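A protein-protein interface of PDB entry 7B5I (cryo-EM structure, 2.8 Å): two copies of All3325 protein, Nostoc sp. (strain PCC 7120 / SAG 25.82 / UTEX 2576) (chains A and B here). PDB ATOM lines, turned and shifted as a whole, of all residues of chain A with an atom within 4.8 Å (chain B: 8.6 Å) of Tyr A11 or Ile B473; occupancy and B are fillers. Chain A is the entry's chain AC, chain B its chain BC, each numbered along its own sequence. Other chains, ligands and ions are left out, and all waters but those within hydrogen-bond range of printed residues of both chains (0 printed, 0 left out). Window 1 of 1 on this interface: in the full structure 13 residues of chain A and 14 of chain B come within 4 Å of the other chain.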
ATOM      1  N   TYR A   5     -17.013  34.348 -26.912  1.00  0.00           N
ATOM      2  CA  TYR A   5     -16.991  32.981 -26.414  1.00  0.00           C
ATOM      3  C   TYR A   5     -17.192  32.049 -27.597  1.00  0.00           C
ATOM      4  O   TYR A   5     -18.281  31.996 -28.174  1.00  0.00           O
ATOM      5  CB  TYR A   5     -18.062  32.778 -25.344  1.00  0.00           C
ATOM      6  CG  TYR A   5     -18.008  33.833 -24.260  1.00  0.00           C
ATOM      7  CD1 TYR A   5     -17.126  33.717 -23.200  1.00  0.00           C
ATOM      8  CD2 TYR A   5     -18.841  34.938 -24.301  1.00  0.00           C
ATOM      9  CE1 TYR A   5     -17.072  34.673 -22.214  1.00  0.00           C
ATOM     10  CE2 TYR A   5     -18.793  35.897 -23.318  1.00  0.00           C
ATOM     11  CZ  TYR A   5     -17.905  35.759 -22.276  1.00  0.00           C
ATOM     12  OH  TYR A   5     -17.846  36.708 -21.284  1.00  0.00           O
ATOM     13  N   LYS A   6     -16.132  31.332 -27.970  1.00  0.00           N
ATOM     14  CA  LYS A   6     -16.145  30.468 -29.142  1.00  0.00           C
ATOM     15  C   LYS A   6     -15.954  28.993 -28.827  1.00  0.00           C
ATOM     16  O   LYS A   6     -16.303  28.156 -29.658  1.00  0.00           O
ATOM     17  CB  LYS A   6     -15.060  30.910 -30.131  1.00  0.00           C
ATOM     18  CG  LYS A   6     -15.278  32.303 -30.682  1.00  0.00           C
ATOM     19  CD  LYS A   6     -14.186  32.697 -31.649  1.00  0.00           C
ATOM     20  CE  LYS A   6     -14.411  34.110 -32.157  1.00  0.00           C
ATOM     21  NZ  LYS A   6     -13.328  34.578 -33.061  1.00  0.00           N
ATOM     22  N   THR A   7     -15.401  28.657 -27.664  1.00  0.00           N
ATOM     23  CA  THR A   7     -15.228  27.271 -27.266  1.00  0.00           C
ATOM     24  C   THR A   7     -16.269  26.917 -26.222  1.00  0.00           C
ATOM     25  O   THR A   7     -16.384  27.628 -25.213  1.00  0.00           O
ATOM     26  CB  THR A   7     -13.831  27.042 -26.709  1.00  0.00           C
ATOM     27  OG1 THR A   7     -12.911  26.902 -27.795  1.00  0.00           O
ATOM     28  CG2 THR A   7     -13.791  25.784 -25.868  1.00  0.00           C
ATOM     29  N   GLY A   9     -17.959  25.531 -23.000  1.00  0.00           N
ATOM     30  CA  GLY A   9     -17.432  25.192 -21.696  1.00  0.00           C
ATOM     31  C   GLY A   9     -17.749  26.261 -20.671  1.00  0.00           C
ATOM     32  O   GLY A   9     -18.669  27.053 -20.835  1.00  0.00           O
ATOM     33  N   VAL A  10     -16.960  26.253 -19.600  1.00  0.00           N
ATOM     34  CA  VAL A  10     -17.147  27.129 -18.449  1.00  0.00           C
ATOM     35  C   VAL A  10     -16.088  28.220 -18.491  1.00  0.00           C
ATOM     36  O   VAL A  10     -14.901  27.933 -18.678  1.00  0.00           O
ATOM     37  CB  VAL A  10     -17.065  26.341 -17.130  1.00  0.00           C
ATOM     38  CG1 VAL A  10     -17.232  27.270 -15.943  1.00  0.00           C
ATOM     39  CG2 VAL A  10     -18.108  25.248 -17.097  1.00  0.00           C
ATOM     40  N   TYR A  11     -16.518  29.467 -18.321  1.00  0.00           N
ATOM     41  CA  TYR A  11     -15.631  30.622 -18.277  1.00  0.00           C
ATOM     42  C   TYR A  11     -15.689  31.263 -16.896  1.00  0.00           C
ATOM     43  O   TYR A  11     -16.763  31.362 -16.296  1.00  0.00           O
ATOM     44  CB  TYR A  11     -16.022  31.644 -19.344  1.00  0.00           C
ATOM     45  CG  TYR A  11     -15.771  31.189 -20.760  1.00  0.00           C
ATOM     46  CD1 TYR A  11     -16.661  30.348 -21.405  1.00  0.00           C
ATOM     47  CD2 TYR A  11     -14.659  31.620 -21.459  1.00  0.00           C
ATOM     48  CE1 TYR A  11     -16.435  29.933 -22.700  1.00  0.00           C
ATOM     49  CE2 TYR A  11     -14.431  31.213 -22.752  1.00  0.00           C
ATOM     50  CZ  TYR A  11     -15.318  30.371 -23.368  1.00  0.00           C
ATOM     51  OH  TYR A  11     -15.082  29.968 -24.657  1.00  0.00           O
ATOM     52  N   ILE A  12     -14.538  31.707 -16.397  1.00  0.00           N
ATOM     53  CA  ILE A  12     -14.414  32.248 -15.046  1.00  0.00           C
ATOM     54  C   ILE A  12     -13.933  33.690 -15.123  1.00  0.00           C
ATOM     55  O   ILE A  12     -12.917  33.975 -15.766  1.00  0.00           O
ATOM     56  CB  ILE A  12     -13.459  31.403 -14.185  1.00  0.00           C
ATOM     57  CG1 ILE A  12     -14.070  30.028 -13.913  1.00  0.00           C
ATOM     58  CG2 ILE A  12     -13.111  32.125 -12.905  1.00  0.00           C
ATOM     59  CD1 ILE A  12     -13.141  29.074 -13.226  1.00  0.00           C
ATOM     60  N   GLU A  13     -14.655  34.590 -14.460  1.00  0.00           N
ATOM     61  CA  GLU A  13     -14.351  36.013 -14.471  1.00  0.00           C
ATOM     62  C   GLU A  13     -14.487  36.584 -13.065  1.00  0.00           C
ATOM     63  O   GLU A  13     -15.336  36.151 -12.285  1.00  0.00           O
ATOM     64  CB  GLU A  13     -15.278  36.756 -15.439  1.00  0.00           C
ATOM     65  CG  GLU A  13     -15.240  36.215 -16.857  1.00  0.00           C
ATOM     66  CD  GLU A  13     -16.137  36.978 -17.802  1.00  0.00           C
ATOM     67  OE1 GLU A  13     -16.779  37.949 -17.355  1.00  0.00           O
ATOM     68  OE2 GLU A  13     -16.199  36.611 -18.993  1.00  0.00           O
ATOM     69  N   ASN B 335      -7.997  25.046 -25.547  1.00  0.00           N
ATOM     70  CA  ASN B 335      -9.130  25.950 -25.753  1.00  0.00           C
ATOM     71  C   ASN B 335      -8.880  26.937 -26.885  1.00  0.00           C
ATOM     72  O   ASN B 335      -9.809  27.267 -27.632  1.00  0.00           O
ATOM     73  CB  ASN B 335      -9.452  26.719 -24.473  1.00  0.00           C
ATOM     74  CG  ASN B 335     -10.218  25.891 -23.469  1.00  0.00           C
ATOM     75  OD1 ASN B 335     -10.809  24.871 -23.811  1.00  0.00           O
ATOM     76  ND2 ASN B 335     -10.232  26.337 -22.221  1.00  0.00           N
ATOM     77  N   GLU B 336      -7.644  27.419 -27.031  1.00  0.00           N
ATOM     78  CA  GLU B 336      -7.374  28.429 -28.047  1.00  0.00           C
ATOM     79  C   GLU B 336      -7.514  27.842 -29.444  1.00  0.00           C
ATOM     80  O   GLU B 336      -7.967  28.522 -30.371  1.00  0.00           O
ATOM     81  CB  GLU B 336      -5.985  29.028 -27.848  1.00  0.00           C
ATOM     82  CG  GLU B 336      -5.728  30.263 -28.707  1.00  0.00           C
ATOM     83  CD  GLU B 336      -4.492  30.158 -29.576  1.00  0.00           C
ATOM     84  OE1 GLU B 336      -3.699  29.216 -29.382  1.00  0.00           O
ATOM     85  OE2 GLU B 336      -4.311  31.028 -30.455  1.00  0.00           O
ATOM     86  N   GLN B 338      -9.498  25.186 -29.994  1.00  0.00           N
ATOM     87  CA  GLN B 338     -10.925  24.909 -30.079  1.00  0.00           C
ATOM     88  C   GLN B 338     -11.696  26.127 -30.558  1.00  0.00           C
ATOM     89  O   GLN B 338     -12.722  25.983 -31.228  1.00  0.00           O
ATOM     90  CB  GLN B 338     -11.448  24.458 -28.718  1.00  0.00           C
ATOM     91  CG  GLN B 338     -12.827  23.811 -28.727  1.00  0.00           C
ATOM     92  CD  GLN B 338     -12.827  22.431 -29.332  1.00  0.00           C
ATOM     93  OE1 GLN B 338     -11.911  21.653 -29.104  1.00  0.00           O
ATOM     94  NE2 GLN B 338     -13.866  22.112 -30.088  1.00  0.00           N
ATOM     95  N   ASN B 339     -11.225  27.331 -30.221  1.00  0.00           N
ATOM     96  CA  ASN B 339     -11.914  28.541 -30.664  1.00  0.00           C
ATOM     97  C   ASN B 339     -11.980  28.632 -32.177  1.00  0.00           C
ATOM     98  O   ASN B 339     -12.988  29.085 -32.728  1.00  0.00           O
ATOM     99  CB  ASN B 339     -11.225  29.782 -30.108  1.00  0.00           C
ATOM    100  CG  ASN B 339     -11.443  29.940 -28.633  1.00  0.00           C
ATOM    101  OD1 ASN B 339     -12.528  30.309 -28.191  1.00  0.00           O
ATOM    102  ND2 ASN B 339     -10.414  29.662 -27.854  1.00  0.00           N
ATOM    103  N   ASN B 342     -14.213  25.493 -33.652  1.00  0.00           N
ATOM    104  CA  ASN B 342     -15.654  25.501 -33.431  1.00  0.00           C
ATOM    105  C   ASN B 342     -16.360  26.588 -34.233  1.00  0.00           C
ATOM    106  O   ASN B 342     -17.481  26.382 -34.704  1.00  0.00           O
ATOM    107  CB  ASN B 342     -15.949  25.663 -31.941  1.00  0.00           C
ATOM    108  CG  ASN B 342     -17.409  25.458 -31.614  1.00  0.00           C
ATOM    109  OD1 ASN B 342     -18.031  24.510 -32.081  1.00  0.00           O
ATOM    110  ND2 ASN B 342     -17.962  26.342 -30.798  1.00  0.00           N
ATOM    111  N   TRP B 364     -16.889  16.490 -27.693  1.00  0.00           N
ATOM    112  CA  TRP B 364     -17.014  17.893 -27.320  1.00  0.00           C
ATOM    113  C   TRP B 364     -17.304  18.673 -28.599  1.00  0.00           C
ATOM    114  O   TRP B 364     -16.387  18.978 -29.368  1.00  0.00           O
ATOM    115  CB  TRP B 364     -15.731  18.358 -26.633  1.00  0.00           C
ATOM    116  CG  TRP B 364     -15.887  19.468 -25.631  1.00  0.00           C
ATOM    117  CD1 TRP B 364     -15.487  20.763 -25.772  1.00  0.00           C
ATOM    118  CD2 TRP B 364     -16.480  19.376 -24.331  1.00  0.00           C
ATOM    119  NE1 TRP B 364     -15.790  21.478 -24.644  1.00  0.00           N
ATOM    120  CE2 TRP B 364     -16.405  20.650 -23.745  1.00  0.00           C
ATOM    121  CE3 TRP B 364     -17.076  18.338 -23.608  1.00  0.00           C
ATOM    122  CZ2 TRP B 364     -16.900  20.915 -22.471  1.00  0.00           C
ATOM    123  CZ3 TRP B 364     -17.566  18.604 -22.345  1.00  0.00           C
ATOM    124  CH2 TRP B 364     -17.474  19.878 -21.790  1.00  0.00           C
ATOM    125  N   ALA B 470     -27.667  24.923 -24.706  1.00  0.00           N
ATOM    126  CA  ALA B 470     -26.825  25.953 -24.111  1.00  0.00           C
ATOM    127  C   ALA B 470     -25.370  25.505 -24.155  1.00  0.00           C
ATOM    128  O   ALA B 470     -25.026  24.459 -23.600  1.00  0.00           O
ATOM    129  CB  ALA B 470     -27.252  26.235 -22.672  1.00  0.00           C
ATOM    130  N   GLU B 471     -24.517  26.300 -24.800  1.00  0.00           N
ATOM    131  CA  GLU B 471     -23.121  25.924 -24.989  1.00  0.00           C
ATOM    132  C   GLU B 471     -22.145  26.604 -24.039  1.00  0.00           C
ATOM    133  O   GLU B 471     -21.070  26.050 -23.799  1.00  0.00           O
ATOM    134  CB  GLU B 471     -22.670  26.222 -26.420  1.00  0.00           C
ATOM    135  CG  GLU B 471     -23.240  25.309 -27.473  1.00  0.00           C
ATOM    136  CD  GLU B 471     -22.734  25.647 -28.854  1.00  0.00           C
ATOM    137  OE1 GLU B 471     -22.639  26.842 -29.187  1.00  0.00           O
ATOM    138  OE2 GLU B 471     -22.414  24.713 -29.610  1.00  0.00           O
ATOM    139  N   PHE B 472     -22.460  27.780 -23.510  1.00  0.00           N
ATOM    140  CA  PHE B 472     -21.473  28.551 -22.768  1.00  0.00           C
ATOM    141  C   PHE B 472     -22.005  28.923 -21.394  1.00  0.00           C
ATOM    142  O   PHE B 472     -23.125  29.423 -21.266  1.00  0.00           O
ATOM    143  CB  PHE B 472     -21.083  29.809 -23.545  1.00  0.00           C
ATOM    144  CG  PHE B 472     -20.708  29.537 -24.973  1.00  0.00           C
ATOM    145  CD1 PHE B 472     -19.514  28.916 -25.284  1.00  0.00           C
ATOM    146  CD2 PHE B 472     -21.550  29.906 -26.003  1.00  0.00           C
ATOM    147  CE1 PHE B 472     -19.176  28.664 -26.591  1.00  0.00           C
ATOM    148  CE2 PHE B 472     -21.213  29.656 -27.310  1.00  0.00           C
ATOM    149  CZ  PHE B 472     -20.027  29.035 -27.603  1.00  0.00           C
ATOM    150  N   ILE B 473     -21.187  28.688 -20.370  1.00  0.00           N
ATOM    151  CA  ILE B 473     -21.535  28.973 -18.983  1.00  0.00           C
ATOM    152  C   ILE B 473     -20.486  29.914 -18.413  1.00  0.00           C
ATOM    153  O   ILE B 473     -19.288  29.626 -18.480  1.00  0.00           O
ATOM    154  CB  ILE B 473     -21.622  27.688 -18.143  1.00  0.00           C
ATOM    155  CG1 ILE B 473     -22.641  26.721 -18.753  1.00  0.00           C
ATOM    156  CG2 ILE B 473     -21.982  28.026 -16.713  1.00  0.00           C
ATOM    157  CD1 ILE B 473     -22.633  25.337 -18.141  1.00  0.00           C
ATOM    158  N   ILE B 474     -20.933  31.033 -17.857  1.00  0.00           N
ATOM    159  CA  ILE B 474     -20.049  32.099 -17.407  1.00  0.00           C
ATOM    160  C   ILE B 474     -20.240  32.292 -15.911  1.00  0.00           C
ATOM    161  O   ILE B 474     -21.357  32.553 -15.456  1.00  0.00           O
ATOM    162  CB  ILE B 474     -20.324  33.404 -18.171  1.00  0.00           C
ATOM    163  CG1 ILE B 474     -20.206  33.156 -19.676  1.00  0.00           C
ATOM    164  CG2 ILE B 474     -19.364  34.484 -17.724  1.00  0.00           C
ATOM    165  CD1 ILE B 474     -20.801  34.236 -20.530  1.00  0.00           C
ATOM    166  N   LEU B 475     -19.155  32.169 -15.153  1.00  0.00           N
ATOM    167  CA  LEU B 475     -19.183  32.349 -13.710  1.00  0.00           C
ATOM    168  C   LEU B 475     -18.449  33.626 -13.328  1.00  0.00           C
ATOM    169  O   LEU B 475     -17.383  33.933 -13.863  1.00  0.00           O
ATOM    170  CB  LEU B 475     -18.543  31.159 -12.992  1.00  0.00           C
ATOM    171  CG  LEU B 475     -19.100  29.769 -13.285  1.00  0.00           C
ATOM    172  CD1 LEU B 475     -18.321  28.724 -12.519  1.00  0.00           C
ATOM    173  CD2 LEU B 475     -20.570  29.689 -12.944  1.00  0.00           C
ATOM    174  N   LYS B 476     -19.014  34.360 -12.377  1.00  0.00           N
ATOM    175  CA  LYS B 476     -18.428  35.609 -11.913  1.00  0.00           C
ATOM    176  C   LYS B 476     -18.292  35.573 -10.401  1.00  0.00           C
ATOM    177  O   LYS B 476     -19.240  35.228  -9.695  1.00  0.00           O
ATOM    178  CB  LYS B 476     -19.278  36.797 -12.337  1.00  0.00           C
ATOM    179  CG  LYS B 476     -19.406  36.935 -13.831  1.00  0.00           C
ATOM    180  CD  LYS B 476     -20.215  38.150 -14.195  1.00  0.00           C
ATOM    181  CE  LYS B 476     -20.333  38.298 -15.693  1.00  0.00           C
ATOM    182  NZ  LYS B 476     -21.143  39.487 -16.053  1.00  0.00           N
ATOM    183  N   PHE B 477     -17.126  35.965  -9.907  1.00  0.00           N
ATOM    184  CA  PHE B 477     -16.801  35.832  -8.496  1.00  0.00           C
ATOM    185  C   PHE B 477     -16.539  37.204  -7.897  1.00  0.00           C
ATOM    186  O   PHE B 477     -16.194  38.155  -8.601  1.00  0.00           O
ATOM    187  CB  PHE B 477     -15.583  34.935  -8.280  1.00  0.00           C
ATOM    188  CG  PHE B 477     -15.815  33.497  -8.639  1.00  0.00           C
ATOM    189  CD1 PHE B 477     -15.671  33.065  -9.945  1.00  0.00           C
ATOM    190  CD2 PHE B 477     -16.151  32.572  -7.670  1.00  0.00           C
ATOM    191  CE1 PHE B 477     -15.877  31.747 -10.281  1.00  0.00           C
ATOM    192  CE2 PHE B 477     -16.356  31.245  -8.003  1.00  0.00           C
ATOM    193  CZ  PHE B 477     -16.221  30.836  -9.310  1.00  0.00           C
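Hydrophobic or aromatic side chains of chain B that line the printed part of chain A: Phe B472, Ile B474, Leu B475 and Phe B477.
Of the 8 printed residues of chain A, 8 touch a printed residue of chain B.
Hydrophobic or aromatic side chains of chain A within 4 Å of the printed part of chain B: Tyr A5, Val A10, Tyr A11 and Ile A12.
Among the printed residues, 22 pairs touch across the chains.
Among the printed residues, no Asp or Glu carboxylate lies within 4 Å of a Lys or Arg side-chain nitrogen of the other chain.
Phe B472 touches Tyr A5 (CZ to O, 3.5 Å).
Tyr A5 touches Ile B474 (CZ to CD1, 3.7 Å).
Lys A6 touches Phe B472.
Thr A7 touches Gln B338.
O of Thr A7 touches CE1 of Phe B472, 3.3 Å away.
Gly A9 touches Phe B472 (O to CA, 3.7 Å).
Val A10 touches Leu B475 (CG1 to CD1, 3.9 Å).
Ile A12 touches Leu B475.
CE1 of Phe B477 touches CG2 of Ile A12, at 3.8 Å.
CA of Lys B476 touches O of Glu A13, 3.2 Å away.
The backbone carbonyl oxygen of Lys A6 is in hydrogen-bond range of the side-chain amide nitrogen of Asn B342 (2.7 Å).
The backbone carbonyl oxygen (O) of Asn B335 sits at hydrogen-bond distance from the side-chain hydroxyl (OG1) of Thr A7 (3.1 Å).
The side-chain hydroxyl (OG1) of Thr A7 sits at hydrogen-bond distance from the backbone NH (N) of Asn B339, 3.0 Å away.
The backbone carbonyl oxygen (O) of Glu B471 lies within hydrogen-bond range of the backbone NH (N) of Gly A9 (3.3 Å).
The backbone carbonyl oxygen (O) of Gly A9 is in hydrogen-bond range of the backbone NH (N) of Ile B473 (3.0 Å).
N of Tyr A11 sits at hydrogen-bond distance from O of Ile B473 (2.8 Å).
N of Leu B475 sits at hydrogen-bond distance from O of Tyr A11 (2.8 Å).
The backbone NH (N) of Glu A13 is in hydrogen-bond range of the backbone carbonyl oxygen (O) of Leu B475 (2.9 Å).
The backbone NH (N) of Phe B477 lies within hydrogen-bond range of the backbone carbonyl oxygen (O) of Glu A13 (3.0 Å).
The side-chain carboxylate (OE2) of Glu A13 lies within hydrogen-bond range of the side-chain hydroxyl (OH) of Tyr A5 (2.8 Å).
The backbone carbonyl oxygen of Thr A7 lies within hydrogen-bond range of the side-chain hydroxyl of Tyr A11.
The side-chain amide nitrogen of Asn B339 sits at hydrogen-bond distance from the backbone carbonyl oxygen of Asn B335, at 2.5 Å.
Printed residues of chain B within 4 Å of Tyr A5: Phe B472 and Ile B474.
Of chain B, only Ile B473 and Leu B475 come within 4 Å of Val A10.
Of chain B, only Ile B473 (2.8 Å), Ile B474 (3.5 Å) and Leu B475 (2.8 Å) come within 4 Å of Tyr A11.
Printed residues of chain A within 4 Å of Asn B335: Thr A7 (3.1 Å).
Printed residues of chain A within 4 Å of Gln B338: Thr A7.
Of the printed residues of chain A, Phe B472 touches Tyr A5, Lys A6, Thr A7 and Gly A9.
Of chain A, only Gly A9, Val A10 and Tyr A11 come within 4 Å of Ile B473.
Printed residues of chain A within 4 Å of Lys B476: Glu A13.
The nearest residue of chain B that does not touch Tyr A11 is Phe B472 (4.1 Å).
The nearest printed residue of chain A that does not touch Ile B473 is Ile A12 (5.6 Å).
The nearest printed residue of chain B that does not touch Thr A7 is Asn B342 (4.6 Å).
No position is printed for both chains.
Of the 22 pairs that touch across the chains among the printed residues, none has its exchanged pair printed and touching as well.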
